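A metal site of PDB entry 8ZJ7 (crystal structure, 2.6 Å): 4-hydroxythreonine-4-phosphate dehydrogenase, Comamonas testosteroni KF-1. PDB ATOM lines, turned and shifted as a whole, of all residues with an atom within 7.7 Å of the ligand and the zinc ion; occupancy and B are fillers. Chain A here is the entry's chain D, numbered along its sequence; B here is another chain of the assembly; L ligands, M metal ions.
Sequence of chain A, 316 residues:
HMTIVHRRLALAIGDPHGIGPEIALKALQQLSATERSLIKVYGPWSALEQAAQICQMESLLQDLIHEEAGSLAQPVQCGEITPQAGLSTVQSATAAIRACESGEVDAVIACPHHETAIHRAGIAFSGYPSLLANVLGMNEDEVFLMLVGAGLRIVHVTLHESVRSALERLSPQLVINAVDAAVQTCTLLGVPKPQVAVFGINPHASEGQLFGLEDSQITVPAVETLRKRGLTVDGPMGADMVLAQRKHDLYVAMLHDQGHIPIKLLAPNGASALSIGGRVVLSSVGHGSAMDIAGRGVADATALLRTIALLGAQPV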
ATOM      1  N   SER A 126       8.714 -29.129 -26.234  1.00  0.00           N
ATOM      2  CA  SER A 126       7.749 -28.062 -26.033  1.00  0.00           C
ATOM      3  C   SER A 126       8.443 -26.709 -26.042  1.00  0.00           C
ATOM      4  O   SER A 126       7.924 -25.762 -25.467  1.00  0.00           O
ATOM      5  CB  SER A 126       6.992 -28.272 -24.746  1.00  0.00           C
ATOM      6  OG  SER A 126       7.908 -28.380 -23.660  1.00  0.00           O
ATOM      7  N   GLY A 127       9.600 -26.618 -26.692  1.00  0.00           N
ATOM      8  CA  GLY A 127      10.376 -25.381 -26.715  1.00  0.00           C
ATOM      9  C   GLY A 127      11.758 -25.546 -26.094  1.00  0.00           C
ATOM     10  O   GLY A 127      12.021 -26.531 -25.411  1.00  0.00           O
ATOM     11  N   TYR A 128      12.618 -24.554 -26.340  1.00  0.00           N
ATOM     12  CA  TYR A 128      14.002 -24.586 -25.927  1.00  0.00           C
ATOM     13  C   TYR A 128      14.120 -24.547 -24.400  1.00  0.00           C
ATOM     14  O   TYR A 128      15.012 -25.186 -23.841  1.00  0.00           O
ATOM     15  CB  TYR A 128      14.760 -23.470 -26.675  1.00  0.00           C
ATOM     16  CG  TYR A 128      15.047 -23.846 -28.122  1.00  0.00           C
ATOM     17  CD1 TYR A 128      15.932 -24.879 -28.420  1.00  0.00           C
ATOM     18  CD2 TYR A 128      14.437 -23.191 -29.181  1.00  0.00           C
ATOM     19  CE1 TYR A 128      16.177 -25.257 -29.734  1.00  0.00           C
ATOM     20  CE2 TYR A 128      14.711 -23.527 -30.503  1.00  0.00           C
ATOM     21  CZ  TYR A 128      15.576 -24.574 -30.773  1.00  0.00           C
ATOM     22  OH  TYR A 128      15.878 -24.955 -32.055  1.00  0.00           O
ATOM     23  N   PRO A 129      13.262 -23.803 -23.665  1.00  0.00           N
ATOM     24  CA  PRO A 129      13.325 -23.860 -22.196  1.00  0.00           C
ATOM     25  C   PRO A 129      13.182 -25.278 -21.636  1.00  0.00           C
ATOM     26  O   PRO A 129      13.888 -25.630 -20.686  1.00  0.00           O
ATOM     27  CB  PRO A 129      12.189 -22.934 -21.755  1.00  0.00           C
ATOM     28  CG  PRO A 129      11.958 -22.001 -22.933  1.00  0.00           C
ATOM     29  CD  PRO A 129      12.280 -22.837 -24.167  1.00  0.00           C
ATOM     30  N   LEU A 145      12.617 -17.766 -19.550  1.00  0.00           N
ATOM     31  CA  LEU A 145      12.637 -17.178 -20.878  1.00  0.00           C
ATOM     32  C   LEU A 145      12.786 -15.666 -20.742  1.00  0.00           C
ATOM     33  O   LEU A 145      11.976 -15.014 -20.093  1.00  0.00           O
ATOM     34  CB  LEU A 145      11.337 -17.474 -21.625  1.00  0.00           C
ATOM     35  CG  LEU A 145      11.256 -16.817 -23.008  1.00  0.00           C
ATOM     36  CD1 LEU A 145      11.992 -17.683 -24.002  1.00  0.00           C
ATOM     37  CD2 LEU A 145       9.842 -16.592 -23.455  1.00  0.00           C
ATOM     38  N   MET A 146      13.797 -15.115 -21.415  1.00  0.00           N
ATOM     39  CA  MET A 146      13.970 -13.675 -21.515  1.00  0.00           C
ATOM     40  C   MET A 146      13.738 -13.237 -22.958  1.00  0.00           C
ATOM     41  O   MET A 146      14.397 -13.713 -23.886  1.00  0.00           O
ATOM     42  CB  MET A 146      15.387 -13.313 -21.044  1.00  0.00           C
ATOM     43  CG  MET A 146      15.818 -11.866 -21.261  1.00  0.00           C
ATOM     44  SD  MET A 146      17.136 -11.441 -20.110  1.00  0.00           S
ATOM     45  CE  MET A 146      18.055 -10.461 -21.308  1.00  0.00           C
ATOM     46  N   LEU A 147      12.779 -12.343 -23.172  1.00  0.00           N
ATOM     47  CA  LEU A 147      12.545 -11.788 -24.493  1.00  0.00           C
ATOM     48  C   LEU A 147      13.355 -10.508 -24.590  1.00  0.00           C
ATOM     49  O   LEU A 147      13.416  -9.729 -23.641  1.00  0.00           O
ATOM     50  CB  LEU A 147      11.063 -11.515 -24.784  1.00  0.00           C
ATOM     51  CG  LEU A 147      10.182 -12.755 -25.000  1.00  0.00           C
ATOM     52  CD1 LEU A 147       8.730 -12.351 -25.200  1.00  0.00           C
ATOM     53  CD2 LEU A 147      10.608 -13.590 -26.176  1.00  0.00           C
ATOM     54  N   HIS A 156      10.642 -13.749 -17.781  1.00  0.00           N
ATOM     55  CA  HIS A 156       9.336 -14.217 -17.358  1.00  0.00           C
ATOM     56  C   HIS A 156       9.506 -15.176 -16.180  1.00  0.00           C
ATOM     57  O   HIS A 156      10.195 -16.171 -16.296  1.00  0.00           O
ATOM     58  CB  HIS A 156       8.601 -14.921 -18.502  1.00  0.00           C
ATOM     59  CG  HIS A 156       8.384 -14.017 -19.643  1.00  0.00           C
ATOM     60  ND1 HIS A 156       9.439 -13.495 -20.355  1.00  0.00           N
ATOM     61  CD2 HIS A 156       7.284 -13.436 -20.127  1.00  0.00           C
ATOM     62  CE1 HIS A 156       8.972 -12.680 -21.289  1.00  0.00           C
ATOM     63  NE2 HIS A 156       7.671 -12.630 -21.177  1.00  0.00           N
ATOM     64  N   LEU A 159       5.455 -18.923 -17.404  1.00  0.00           N
ATOM     65  CA  LEU A 159       5.332 -19.028 -18.836  1.00  0.00           C
ATOM     66  C   LEU A 159       4.478 -20.238 -19.146  1.00  0.00           C
ATOM     67  O   LEU A 159       4.656 -21.295 -18.542  1.00  0.00           O
ATOM     68  CB  LEU A 159       6.743 -19.218 -19.391  1.00  0.00           C
ATOM     69  CG  LEU A 159       6.904 -19.098 -20.909  1.00  0.00           C
ATOM     70  CD1 LEU A 159       7.040 -17.637 -21.229  1.00  0.00           C
ATOM     71  CD2 LEU A 159       8.102 -19.906 -21.378  1.00  0.00           C
ATOM     72  N   HIS A 160       3.591 -20.133 -20.114  1.00  0.00           N
ATOM     73  CA  HIS A 160       2.897 -21.286 -20.685  1.00  0.00           C
ATOM     74  C   HIS A 160       2.240 -22.166 -19.623  1.00  0.00           C
ATOM     75  O   HIS A 160       2.560 -23.330 -19.481  1.00  0.00           O
ATOM     76  CB  HIS A 160       3.775 -22.117 -21.623  1.00  0.00           C
ATOM     77  CG  HIS A 160       4.164 -21.315 -22.812  1.00  0.00           C
ATOM     78  ND1 HIS A 160       5.403 -21.441 -23.385  1.00  0.00           N
ATOM     79  CD2 HIS A 160       3.528 -20.323 -23.463  1.00  0.00           C
ATOM     80  CE1 HIS A 160       5.491 -20.561 -24.374  1.00  0.00           C
ATOM     81  NE2 HIS A 160       4.363 -19.870 -24.438  1.00  0.00           N
ATOM     82  N   HIS A 256       3.024 -14.540 -18.504  1.00  0.00           N
ATOM     83  CA  HIS A 256       3.317 -14.620 -19.919  1.00  0.00           C
ATOM     84  C   HIS A 256       2.946 -13.312 -20.612  1.00  0.00           C
ATOM     85  O   HIS A 256       3.802 -12.665 -21.202  1.00  0.00           O
ATOM     86  CB  HIS A 256       2.574 -15.835 -20.473  1.00  0.00           C
ATOM     87  CG  HIS A 256       2.727 -16.056 -21.949  1.00  0.00           C
ATOM     88  ND1 HIS A 256       1.950 -15.376 -22.870  1.00  0.00           N
ATOM     89  CD2 HIS A 256       3.519 -16.883 -22.652  1.00  0.00           C
ATOM     90  CE1 HIS A 256       2.290 -15.774 -24.091  1.00  0.00           C
ATOM     91  NE2 HIS A 256       3.229 -16.700 -23.989  1.00  0.00           N
ATOM     92  N   ASP A 257       1.679 -12.909 -20.518  1.00  0.00           N
ATOM     93  CA  ASP A 257       1.127 -11.838 -21.336  1.00  0.00           C
ATOM     94  C   ASP A 257       1.774 -10.493 -20.986  1.00  0.00           C
ATOM     95  O   ASP A 257       1.917  -9.626 -21.846  1.00  0.00           O
ATOM     96  CB  ASP A 257      -0.395 -11.822 -21.249  1.00  0.00           C
ATOM     97  CG  ASP A 257      -1.149 -12.896 -22.028  1.00  0.00           C
ATOM     98  OD1 ASP A 257      -0.507 -13.731 -22.729  1.00  0.00           O
ATOM     99  OD2 ASP A 257      -2.403 -12.912 -21.926  1.00  0.00           O
ATOM    100  N   HIS A 260       5.021 -10.598 -22.999  1.00  0.00           N
ATOM    101  CA  HIS A 260       4.948 -10.903 -24.405  1.00  0.00           C
ATOM    102  C   HIS A 260       4.343  -9.753 -25.188  1.00  0.00           C
ATOM    103  O   HIS A 260       4.728  -9.546 -26.337  1.00  0.00           O
ATOM    104  CB  HIS A 260       4.177 -12.210 -24.664  1.00  0.00           C
ATOM    105  CG  HIS A 260       5.012 -13.431 -24.493  1.00  0.00           C
ATOM    106  ND1 HIS A 260       5.736 -13.690 -23.342  1.00  0.00           N
ATOM    107  CD2 HIS A 260       5.241 -14.458 -25.315  1.00  0.00           C
ATOM    108  CE1 HIS A 260       6.382 -14.838 -23.482  1.00  0.00           C
ATOM    109  NE2 HIS A 260       6.095 -15.324 -24.677  1.00  0.00           N
ATOM    110  N   LYS A 264       6.132  -8.009 -28.728  1.00  0.00           N
ATOM    111  CA  LYS A 264       5.525  -8.253 -30.029  1.00  0.00           C
ATOM    112  C   LYS A 264       5.103  -6.937 -30.681  1.00  0.00           C
ATOM    113  O   LYS A 264       5.142  -6.834 -31.919  1.00  0.00           O
ATOM    114  CB  LYS A 264       4.235  -9.073 -30.000  1.00  0.00           C
ATOM    115  CG  LYS A 264       4.337 -10.538 -29.629  1.00  0.00           C
ATOM    116  CD  LYS A 264       4.959 -11.469 -30.680  1.00  0.00           C
ATOM    117  CE  LYS A 264       4.302 -12.850 -30.729  1.00  0.00           C
ATOM    118  NZ  LYS A 264       4.108 -13.536 -29.436  1.00  0.00           N
ATOM    119  N   SER A 272      14.391 -11.396 -29.915  1.00  0.00           N
ATOM    120  CA  SER A 272      15.139 -12.596 -29.593  1.00  0.00           C
ATOM    121  C   SER A 272      14.481 -13.247 -28.371  1.00  0.00           C
ATOM    122  O   SER A 272      13.987 -12.557 -27.485  1.00  0.00           O
ATOM    123  CB  SER A 272      16.614 -12.294 -29.349  1.00  0.00           C
ATOM    124  OG  SER A 272      17.286 -11.907 -30.533  1.00  0.00           O
ATOM    125  N   ALA A 273      14.498 -14.580 -28.338  1.00  0.00           N
ATOM    126  CA  ALA A 273      14.052 -15.330 -27.168  1.00  0.00           C
ATOM    127  C   ALA A 273      15.244 -16.073 -26.585  1.00  0.00           C
ATOM    128  O   ALA A 273      15.777 -16.976 -27.249  1.00  0.00           O
ATOM    129  CB  ALA A 273      12.939 -16.293 -27.563  1.00  0.00           C
ATOM    130  N   LEU A 274      15.680 -15.692 -25.386  1.00  0.00           N
ATOM    131  CA  LEU A 274      16.796 -16.363 -24.730  1.00  0.00           C
ATOM    132  C   LEU A 274      16.256 -17.319 -23.672  1.00  0.00           C
ATOM    133  O   LEU A 274      15.497 -16.916 -22.785  1.00  0.00           O
ATOM    134  CB  LEU A 274      17.748 -15.350 -24.102  1.00  0.00           C
ATOM    135  CG  LEU A 274      18.125 -14.131 -24.949  1.00  0.00           C
ATOM    136  CD1 LEU A 274      19.364 -13.447 -24.356  1.00  0.00           C
ATOM    137  CD2 LEU A 274      18.425 -14.444 -26.387  1.00  0.00           C
ATOM    138  N   SER A 275      16.644 -18.593 -23.742  1.00  0.00           N
ATOM    139  CA  SER A 275      16.386 -19.518 -22.660  1.00  0.00           C
ATOM    140  C   SER A 275      17.590 -19.514 -21.720  1.00  0.00           C
ATOM    141  O   SER A 275      18.711 -19.652 -22.207  1.00  0.00           O
ATOM    142  CB  SER A 275      16.088 -20.908 -23.185  1.00  0.00           C
ATOM    143  OG  SER A 275      14.956 -20.888 -24.055  1.00  0.00           O
ATOM    144  N   SER A 284      17.203 -18.744 -29.958  1.00  0.00           N
ATOM    145  CA  SER A 284      16.882 -19.175 -31.309  1.00  0.00           C
ATOM    146  C   SER A 284      17.047 -17.974 -32.238  1.00  0.00           C
ATOM    147  O   SER A 284      17.313 -16.879 -31.778  1.00  0.00           O
ATOM    148  CB  SER A 284      15.514 -19.825 -31.404  1.00  0.00           C
ATOM    149  OG  SER A 284      14.584 -19.021 -30.703  1.00  0.00           O
ATOM    150  N   PRO B 203      -2.543 -17.632 -21.517  1.00  0.00           N
ATOM    151  CA  PRO B 203      -1.659 -17.523 -22.675  1.00  0.00           C
ATOM    152  C   PRO B 203      -2.140 -18.363 -23.855  1.00  0.00           C
ATOM    153  O   PRO B 203      -2.634 -19.474 -23.654  1.00  0.00           O
ATOM    154  CB  PRO B 203      -0.329 -18.052 -22.124  1.00  0.00           C
ATOM    155  CG  PRO B 203      -0.397 -17.813 -20.647  1.00  0.00           C
ATOM    156  CD  PRO B 203      -1.853 -18.005 -20.284  1.00  0.00           C
ATOM    157  N   HIS B 204      -1.996 -17.819 -25.071  1.00  0.00           N
ATOM    158  CA  HIS B 204      -2.361 -18.500 -26.299  1.00  0.00           C
ATOM    159  C   HIS B 204      -3.838 -18.894 -26.300  1.00  0.00           C
ATOM    160  O   HIS B 204      -4.218 -19.859 -26.936  1.00  0.00           O
ATOM    161  CB  HIS B 204      -1.508 -19.753 -26.520  1.00  0.00           C
ATOM    162  CG  HIS B 204      -0.050 -19.484 -26.602  1.00  0.00           C
ATOM    163  ND1 HIS B 204       0.884 -20.323 -26.035  1.00  0.00           N
ATOM    164  CD2 HIS B 204       0.649 -18.505 -27.195  1.00  0.00           C
ATOM    165  CE1 HIS B 204       2.096 -19.863 -26.285  1.00  0.00           C
ATOM    166  NE2 HIS B 204       1.984 -18.756 -26.976  1.00  0.00           N
ATOM    167  N   GLU B 207      -4.688 -22.465 -25.718  1.00  0.00           N
ATOM    168  CA  GLU B 207      -4.317 -23.428 -26.751  1.00  0.00           C
ATOM    169  C   GLU B 207      -5.232 -24.646 -26.696  1.00  0.00           C
ATOM    170  O   GLU B 207      -4.798 -25.761 -26.414  1.00  0.00           O
ATOM    171  CB  GLU B 207      -2.841 -23.837 -26.666  1.00  0.00           C
ATOM    172  CG  GLU B 207      -2.036 -23.306 -27.850  1.00  0.00           C
ATOM    173  CD  GLU B 207      -0.614 -23.813 -28.006  1.00  0.00           C
ATOM    174  OE1 GLU B 207      -0.450 -25.044 -28.012  1.00  0.00           O
ATOM    175  OE2 GLU B 207       0.304 -22.975 -28.141  1.00  0.00           O
ATOM    176  N   PHE B 211      -3.630 -25.135 -21.515  1.00  0.00           N
ATOM    177  CA  PHE B 211      -3.192 -24.233 -20.455  1.00  0.00           C
ATOM    178  C   PHE B 211      -4.406 -23.730 -19.683  1.00  0.00           C
ATOM    179  O   PHE B 211      -4.521 -22.529 -19.440  1.00  0.00           O
ATOM    180  CB  PHE B 211      -2.400 -23.039 -20.998  1.00  0.00           C
ATOM    181  CG  PHE B 211      -1.177 -23.398 -21.842  1.00  0.00           C
ATOM    182  CD1 PHE B 211      -0.339 -24.447 -21.493  1.00  0.00           C
ATOM    183  CD2 PHE B 211      -0.895 -22.670 -23.005  1.00  0.00           C
ATOM    184  CE1 PHE B 211       0.718 -24.786 -22.296  1.00  0.00           C
ATOM    185  CE2 PHE B 211       0.182 -23.011 -23.794  1.00  0.00           C
ATOM    186  CZ  PHE B 211       0.990 -24.058 -23.445  1.00  0.00           C
ATOM    187  N   ASP B 240      -0.992 -10.938 -27.065  1.00  0.00           N
ATOM    188  CA  ASP B 240       0.261 -10.526 -27.685  1.00  0.00           C
ATOM    189  C   ASP B 240       0.189 -10.666 -29.202  1.00  0.00           C
ATOM    190  O   ASP B 240       0.685  -9.788 -29.926  1.00  0.00           O
ATOM    191  CB  ASP B 240       1.427 -11.324 -27.128  1.00  0.00           C
ATOM    192  CG  ASP B 240       1.224 -12.840 -27.084  1.00  0.00           C
ATOM    193  OD1 ASP B 240       0.061 -13.288 -27.087  1.00  0.00           O
ATOM    194  OD2 ASP B 240       2.232 -13.574 -27.074  1.00  0.00           O
ATOM    195  N   MET B 241      -0.414 -11.761 -29.675  1.00  0.00           N
ATOM    196  CA  MET B 241      -0.451 -12.090 -31.085  1.00  0.00           C
ATOM    197  C   MET B 241      -1.392 -11.160 -31.838  1.00  0.00           C
ATOM    198  O   MET B 241      -1.014 -10.617 -32.874  1.00  0.00           O
ATOM    199  CB  MET B 241      -0.894 -13.545 -31.323  1.00  0.00           C
ATOM    200  CG  MET B 241      -0.428 -14.065 -32.661  1.00  0.00           C
ATOM    201  SD  MET B 241       0.122 -15.787 -32.629  1.00  0.00           S
ATOM    202  CE  MET B 241      -1.426 -16.637 -32.943  1.00  0.00           C
HETATM  203  C1  LIG L   1       6.660 -17.657 -27.484  1.00  0.00           C
HETATM  204  C2  LIG L   1       6.907 -18.531 -26.428  1.00  0.00           C
HETATM  205  C3  LIG L   1       8.210 -18.757 -26.014  1.00  0.00           C
HETATM  206  O1  LIG L   1       8.451 -19.602 -24.976  1.00  0.00           O
HETATM  207  C4  LIG L   1       9.260 -18.088 -26.654  1.00  0.00           C
HETATM  208  O2  LIG L   1      10.570 -18.271 -26.306  1.00  0.00           O
HETATM  209  C5  LIG L   1       9.020 -17.215 -27.692  1.00  0.00           C
HETATM  210  C6  LIG L   1       7.723 -17.010 -28.108  1.00  0.00           C
HETATM  211  C7  LIG L   1       5.273 -17.411 -27.962  1.00  0.00           C
HETATM  212  O3  LIG L   1       5.134 -16.470 -28.756  1.00  0.00           O
HETATM  213  O4  LIG L   1       4.346 -18.225 -27.608  1.00  0.00           O
HETATM  214 ZN    ZN M   1       4.046 -18.160 -25.647  1.00  0.00          ZN
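O3 of the ligand is in salt-bridge range of NZ of Lys 264, 3.2 Å away.
ND1 of His 256 is in hydrogen-bond range of OD1 of Asp 257. ND1 of His 204 of chain B is in hydrogen-bond range of OE2 of Glu 207 of chain B (3.4 Å). The backbone carbonyl oxygen (O) of His 256 lies within hydrogen-bond range of a ring nitrogen (ND1) of His 260, at 3.1 Å. A ring nitrogen (ND1) of His 260 sits at hydrogen-bond distance from a ring nitrogen (NE2) of His 156 (3.1 Å). NZ of Lys 264 is in salt-bridge range of OD2 of Asp 240 of chain B, at 3.0 Å. The backbone carbonyl oxygen of Leu 145 is in hydrogen-bond range of the backbone NH of His 156, at 3.0 Å.
Leu 145 touches the ligand (CD1 to O2, 2.8 Å). Leu 159 touches the ligand (CD2 to O1, 3.6 Å). NE2 of His 260 touches C1 of the ligand, 3.7 Å away. Ala 273 touches the ligand. Of the 25 residues printed, 7 come within 4 Å of the ligand. The nearest printed residue that does not touch the ligand is His 256 (4.1 Å).
Residues that only touch the zinc ion: His 260 (3.6 Å). Within 4 Å of the zinc ion: His 160, His 256, His 260 and His 204 of chain B.
The zinc ion is bound by an oxygen (O4) of the ligand (2.0 Å), a ring nitrogen (NE2) of His 160 (2.1 Å), a ring nitrogen (NE2) of His 256 (2.4 Å) and a ring nitrogen (NE2) of His 204 of chain B (2.5 Å).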
